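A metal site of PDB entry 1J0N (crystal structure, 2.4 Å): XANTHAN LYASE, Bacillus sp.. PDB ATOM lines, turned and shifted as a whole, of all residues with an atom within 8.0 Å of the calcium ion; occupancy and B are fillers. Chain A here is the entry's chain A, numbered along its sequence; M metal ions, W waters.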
ATOM      1  N   TYR A 466     -40.198  -2.845 -20.403  1.00  0.00           N
ATOM      2  CA  TYR A 466     -39.071  -2.504 -19.544  1.00  0.00           C
ATOM      3  C   TYR A 466     -39.426  -1.277 -18.731  1.00  0.00           C
ATOM      4  O   TYR A 466     -40.437  -0.627 -19.004  1.00  0.00           O
ATOM      5  CB  TYR A 466     -37.824  -2.226 -20.381  1.00  0.00           C
ATOM      6  CG  TYR A 466     -37.555  -3.267 -21.443  1.00  0.00           C
ATOM      7  CD1 TYR A 466     -38.089  -3.143 -22.730  1.00  0.00           C
ATOM      8  CD2 TYR A 466     -36.776  -4.394 -21.160  1.00  0.00           C
ATOM      9  CE1 TYR A 466     -37.862  -4.128 -23.712  1.00  0.00           C
ATOM     10  CE2 TYR A 466     -36.535  -5.379 -22.139  1.00  0.00           C
ATOM     11  CZ  TYR A 466     -37.080  -5.230 -23.413  1.00  0.00           C
ATOM     12  OH  TYR A 466     -36.835  -6.180 -24.380  1.00  0.00           O
ATOM     13  N   PHE A 489     -34.470  -4.491 -17.107  1.00  0.00           N
ATOM     14  CA  PHE A 489     -34.302  -4.821 -18.512  1.00  0.00           C
ATOM     15  C   PHE A 489     -34.877  -6.217 -18.779  1.00  0.00           C
ATOM     16  O   PHE A 489     -35.909  -6.577 -18.213  1.00  0.00           O
ATOM     17  CB  PHE A 489     -32.821  -4.757 -18.881  1.00  0.00           C
ATOM     18  CG  PHE A 489     -32.245  -3.371 -18.820  1.00  0.00           C
ATOM     19  CD1 PHE A 489     -31.105  -3.107 -18.078  1.00  0.00           C
ATOM     20  CD2 PHE A 489     -32.839  -2.327 -19.520  1.00  0.00           C
ATOM     21  CE1 PHE A 489     -30.567  -1.826 -18.021  1.00  0.00           C
ATOM     22  CE2 PHE A 489     -32.307  -1.030 -19.476  1.00  0.00           C
ATOM     23  CZ  PHE A 489     -31.175  -0.784 -18.723  1.00  0.00           C
ATOM     24  N   ASP A 490     -34.207  -7.003 -19.617  1.00  0.00           N
ATOM     25  CA  ASP A 490     -34.697  -8.343 -19.940  1.00  0.00           C
ATOM     26  C   ASP A 490     -34.244  -9.424 -18.952  1.00  0.00           C
ATOM     27  O   ASP A 490     -35.055 -10.217 -18.504  1.00  0.00           O
ATOM     28  CB  ASP A 490     -34.296  -8.731 -21.365  1.00  0.00           C
ATOM     29  CG  ASP A 490     -32.772  -8.750 -21.560  1.00  0.00           C
ATOM     30  OD1 ASP A 490     -32.089  -7.796 -21.128  1.00  0.00           O
ATOM     31  OD2 ASP A 490     -32.250  -9.726 -22.162  1.00  0.00           O
ATOM     32  N   ASP A 491     -32.957  -9.445 -18.601  1.00  0.00           N
ATOM     33  CA  ASP A 491     -32.473 -10.477 -17.690  1.00  0.00           C
ATOM     34  C   ASP A 491     -31.578  -9.960 -16.562  1.00  0.00           C
ATOM     35  O   ASP A 491     -30.931 -10.743 -15.865  1.00  0.00           O
ATOM     36  CB  ASP A 491     -31.745 -11.576 -18.491  1.00  0.00           C
ATOM     37  CG  ASP A 491     -30.461 -11.094 -19.106  1.00  0.00           C
ATOM     38  OD1 ASP A 491     -30.463 -10.001 -19.706  1.00  0.00           O
ATOM     39  OD2 ASP A 491     -29.445 -11.815 -18.998  1.00  0.00           O
ATOM     40  N   GLU A 492     -31.529  -8.647 -16.398  1.00  0.00           N
ATOM     41  CA  GLU A 492     -30.730  -8.062 -15.321  1.00  0.00           C
ATOM     42  C   GLU A 492     -31.403  -6.804 -14.791  1.00  0.00           C
ATOM     43  O   GLU A 492     -32.070  -6.087 -15.530  1.00  0.00           O
ATOM     44  CB  GLU A 492     -29.322  -7.729 -15.805  1.00  0.00           C
ATOM     45  CG  GLU A 492     -29.197  -6.492 -16.688  1.00  0.00           C
ATOM     46  CD  GLU A 492     -29.509  -6.757 -18.159  1.00  0.00           C
ATOM     47  OE1 GLU A 492     -30.686  -6.646 -18.557  1.00  0.00           O
ATOM     48  OE2 GLU A 492     -28.562  -7.092 -18.917  1.00  0.00           O
ATOM     49  N   ILE A 493     -31.221  -6.552 -13.501  1.00  0.00           N
ATOM     50  CA  ILE A 493     -31.766  -5.354 -12.858  1.00  0.00           C
ATOM     51  C   ILE A 493     -30.575  -4.559 -12.327  1.00  0.00           C
ATOM     52  O   ILE A 493     -29.790  -5.068 -11.520  1.00  0.00           O
ATOM     53  CB  ILE A 493     -32.715  -5.699 -11.685  1.00  0.00           C
ATOM     54  CG1 ILE A 493     -33.938  -6.440 -12.207  1.00  0.00           C
ATOM     55  CG2 ILE A 493     -33.132  -4.443 -10.950  1.00  0.00           C
ATOM     56  CD1 ILE A 493     -33.700  -7.907 -12.429  1.00  0.00           C
ATOM     57  N   VAL A 618     -25.578  -5.073 -10.339  1.00  0.00           N
ATOM     58  CA  VAL A 618     -26.540  -5.648 -11.281  1.00  0.00           C
ATOM     59  C   VAL A 618     -26.932  -7.042 -10.780  1.00  0.00           C
ATOM     60  O   VAL A 618     -26.072  -7.855 -10.459  1.00  0.00           O
ATOM     61  CB  VAL A 618     -25.928  -5.783 -12.697  1.00  0.00           C
ATOM     62  CG1 VAL A 618     -27.022  -6.045 -13.709  1.00  0.00           C
ATOM     63  CG2 VAL A 618     -25.171  -4.517 -13.065  1.00  0.00           C
ATOM     64  N   LEU A 620     -28.302 -10.666 -11.374  1.00  0.00           N
ATOM     65  CA  LEU A 620     -28.380 -11.607 -12.484  1.00  0.00           C
ATOM     66  C   LEU A 620     -29.030 -12.909 -12.059  1.00  0.00           C
ATOM     67  O   LEU A 620     -28.352 -13.849 -11.676  1.00  0.00           O
ATOM     68  CB  LEU A 620     -26.979 -11.890 -13.037  1.00  0.00           C
ATOM     69  CG  LEU A 620     -26.254 -10.651 -13.566  1.00  0.00           C
ATOM     70  CD1 LEU A 620     -24.815 -11.000 -13.921  1.00  0.00           C
ATOM     71  CD2 LEU A 620     -27.007 -10.131 -14.790  1.00  0.00           C
ATOM     72  N   LYS A 623     -28.504 -17.503 -13.264  1.00  0.00           N
ATOM     73  CA  LYS A 623     -27.299 -17.753 -14.052  1.00  0.00           C
ATOM     74  C   LYS A 623     -26.315 -18.578 -13.252  1.00  0.00           C
ATOM     75  O   LYS A 623     -26.316 -18.520 -12.022  1.00  0.00           O
ATOM     76  CB  LYS A 623     -26.635 -16.441 -14.478  1.00  0.00           C
ATOM     77  CG  LYS A 623     -27.401 -15.734 -15.566  1.00  0.00           C
ATOM     78  CD  LYS A 623     -26.634 -14.579 -16.167  1.00  0.00           C
ATOM     79  CE  LYS A 623     -27.355 -14.085 -17.408  1.00  0.00           C
ATOM     80  NZ  LYS A 623     -28.807 -13.871 -17.119  1.00  0.00           N
ATOM     81  N   TYR A 631     -20.569 -12.740 -18.045  1.00  0.00           N
ATOM     82  CA  TYR A 631     -21.227 -11.441 -18.033  1.00  0.00           C
ATOM     83  C   TYR A 631     -20.285 -10.344 -17.543  1.00  0.00           C
ATOM     84  O   TYR A 631     -20.192  -9.276 -18.157  1.00  0.00           O
ATOM     85  CB  TYR A 631     -22.452 -11.476 -17.117  1.00  0.00           C
ATOM     86  CG  TYR A 631     -23.320 -10.254 -17.257  1.00  0.00           C
ATOM     87  CD1 TYR A 631     -24.353 -10.219 -18.185  1.00  0.00           C
ATOM     88  CD2 TYR A 631     -23.069  -9.109 -16.509  1.00  0.00           C
ATOM     89  CE1 TYR A 631     -25.127  -9.070 -18.362  1.00  0.00           C
ATOM     90  CE2 TYR A 631     -23.837  -7.958 -16.679  1.00  0.00           C
ATOM     91  CZ  TYR A 631     -24.862  -7.944 -17.607  1.00  0.00           C
ATOM     92  OH  TYR A 631     -25.622  -6.814 -17.776  1.00  0.00           O
ATOM     93  N   PRO A 635     -19.940  -7.296 -20.179  1.00  0.00           N
ATOM     94  CA  PRO A 635     -21.292  -6.912 -19.746  1.00  0.00           C
ATOM     95  C   PRO A 635     -22.163  -6.174 -20.763  1.00  0.00           C
ATOM     96  O   PRO A 635     -21.682  -5.326 -21.518  1.00  0.00           O
ATOM     97  CB  PRO A 635     -21.012  -6.043 -18.523  1.00  0.00           C
ATOM     98  CG  PRO A 635     -19.742  -5.355 -18.904  1.00  0.00           C
ATOM     99  CD  PRO A 635     -18.922  -6.484 -19.494  1.00  0.00           C
ATOM    100  N   ALA A 636     -23.448  -6.519 -20.772  1.00  0.00           N
ATOM    101  CA  ALA A 636     -24.388  -5.883 -21.680  1.00  0.00           C
ATOM    102  C   ALA A 636     -24.826  -4.549 -21.068  1.00  0.00           C
ATOM    103  O   ALA A 636     -25.586  -3.790 -21.671  1.00  0.00           O
ATOM    104  CB  ALA A 636     -25.591  -6.792 -21.894  1.00  0.00           C
ATOM    105  N   ILE A 637     -24.324  -4.264 -19.880  1.00  0.00           N
ATOM    106  CA  ILE A 637     -24.674  -3.036 -19.200  1.00  0.00           C
ATOM    107  C   ILE A 637     -23.537  -2.029 -19.250  1.00  0.00           C
ATOM    108  O   ILE A 637     -22.366  -2.384 -19.384  1.00  0.00           O
ATOM    109  CB  ILE A 637     -25.110  -3.326 -17.740  1.00  0.00           C
ATOM    110  CG1 ILE A 637     -26.538  -2.829 -17.554  1.00  0.00           C
ATOM    111  CG2 ILE A 637     -24.168  -2.667 -16.729  1.00  0.00           C
ATOM    112  CD1 ILE A 637     -27.483  -3.322 -18.637  1.00  0.00           C
ATOM    113  N   GLU A 651     -28.385  -0.388 -22.108  1.00  0.00           N
ATOM    114  CA  GLU A 651     -28.353  -1.828 -22.348  1.00  0.00           C
ATOM    115  C   GLU A 651     -27.872  -2.023 -23.789  1.00  0.00           C
ATOM    116  O   GLU A 651     -28.666  -2.031 -24.719  1.00  0.00           O
ATOM    117  CB  GLU A 651     -29.730  -2.433 -22.143  1.00  0.00           C
ATOM    118  CG  GLU A 651     -29.730  -3.824 -21.492  1.00  0.00           C
ATOM    119  CD  GLU A 651     -29.088  -4.909 -22.348  1.00  0.00           C
ATOM    120  OE1 GLU A 651     -29.088  -6.071 -21.908  1.00  0.00           O
ATOM    121  OE2 GLU A 651     -28.604  -4.608 -23.461  1.00  0.00           O
ATOM    122  N   LYS A 652     -26.562  -2.168 -23.950  1.00  0.00           N
ATOM    123  CA  LYS A 652     -25.922  -2.325 -25.266  1.00  0.00           C
ATOM    124  C   LYS A 652     -26.669  -3.192 -26.272  1.00  0.00           C
ATOM    125  O   LYS A 652     -26.834  -2.786 -27.422  1.00  0.00           O
ATOM    126  CB  LYS A 652     -24.520  -2.912 -25.092  1.00  0.00           C
ATOM    127  CG  LYS A 652     -23.527  -2.052 -24.351  1.00  0.00           C
ATOM    128  CD  LYS A 652     -22.413  -2.939 -23.788  1.00  0.00           C
ATOM    129  CE  LYS A 652     -21.195  -2.148 -23.342  1.00  0.00           C
ATOM    130  NZ  LYS A 652     -20.458  -1.568 -24.499  1.00  0.00           N
ATOM    131  N   THR A 653     -27.117  -4.368 -25.846  1.00  0.00           N
ATOM    132  CA  THR A 653     -27.791  -5.297 -26.747  1.00  0.00           C
ATOM    133  C   THR A 653     -29.255  -4.994 -27.099  1.00  0.00           C
ATOM    134  O   THR A 653     -29.712  -5.332 -28.189  1.00  0.00           O
ATOM    135  CB  THR A 653     -27.706  -6.766 -26.216  1.00  0.00           C
ATOM    136  OG1 THR A 653     -28.678  -6.963 -25.174  1.00  0.00           O
ATOM    137  CG2 THR A 653     -26.318  -7.035 -25.647  1.00  0.00           C
ATOM    138  N   LEU A 654     -29.993  -4.373 -26.185  1.00  0.00           N
ATOM    139  CA  LEU A 654     -31.399  -4.052 -26.444  1.00  0.00           C
ATOM    140  C   LEU A 654     -31.578  -2.667 -27.047  1.00  0.00           C
ATOM    141  O   LEU A 654     -32.648  -2.347 -27.551  1.00  0.00           O
ATOM    142  CB  LEU A 654     -32.231  -4.155 -25.162  1.00  0.00           C
ATOM    143  CG  LEU A 654     -32.564  -5.521 -24.533  1.00  0.00           C
ATOM    144  CD1 LEU A 654     -33.295  -6.372 -25.557  1.00  0.00           C
ATOM    145  CD2 LEU A 654     -31.313  -6.212 -24.083  1.00  0.00           C
ATOM    146  N   LEU A 656     -31.368  -0.020 -25.266  1.00  0.00           N
ATOM    147  CA  LEU A 656     -32.082   0.659 -24.194  1.00  0.00           C
ATOM    148  C   LEU A 656     -31.251   1.667 -23.411  1.00  0.00           C
ATOM    149  O   LEU A 656     -30.095   1.413 -23.070  1.00  0.00           O
ATOM    150  CB  LEU A 656     -32.650  -0.374 -23.224  1.00  0.00           C
ATOM    151  CG  LEU A 656     -33.880  -1.131 -23.697  1.00  0.00           C
ATOM    152  CD1 LEU A 656     -34.188  -2.257 -22.719  1.00  0.00           C
ATOM    153  CD2 LEU A 656     -35.056  -0.171 -23.807  1.00  0.00           C
HETATM  154 CA    CA M   1     -29.509  -8.091 -20.782  1.00  0.00          CA
HETATM  155  O   HOH W   1     -29.800  -8.918 -23.073  1.00  0.00           O
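N of Thr 653 sits at hydrogen-bond distance from OE2 of Glu 651 (2.8 Å).
The backbone NH (N) of Leu 654 sits at hydrogen-bond distance from the side-chain carboxylate (OE2) of Glu 651 (3.1 Å).
The side-chain carboxylate of Glu 492 lies close to the side-chain hydroxyl of Tyr 631, at 3.2 Å.
The backbone NH of Glu 651 lies within hydrogen-bond range of the backbone carbonyl oxygen of Leu 656 (2.7 Å).
The side-chain carboxylate of Asp 491 lies within salt-bridge range of the side-chain amino group of Lys 623, at 2.9 Å.
Within 4 Å of the calcium ion: Asp 490, Asp 491, Glu 492 and Glu 651.
The nearest printed residue that does not touch the calcium ion is Leu 654 (4.2 Å).
OE2 of Glu 492 binds the calcium ion.
The calcium ion is bound by OE1 of Glu 651 (2.4 Å).
The calcium ion is bound by the side-chain carboxylate (OD1) of Asp 491, at 2.4 Å.
The calcium ion is bound by water W1 (2.5 Å).
OD1 of Asp 490 is bound to the calcium ion, 2.6 Å away.
The calcium ion has five donor atoms within binding distance.
Slightly farther from the calcium ion lies the side-chain carboxylate (OE1) of Glu 492 (2.9 Å).
Water W1 lies within hydrogen-bond range of OD2 of Asp 490 and OG1 of Thr 653.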
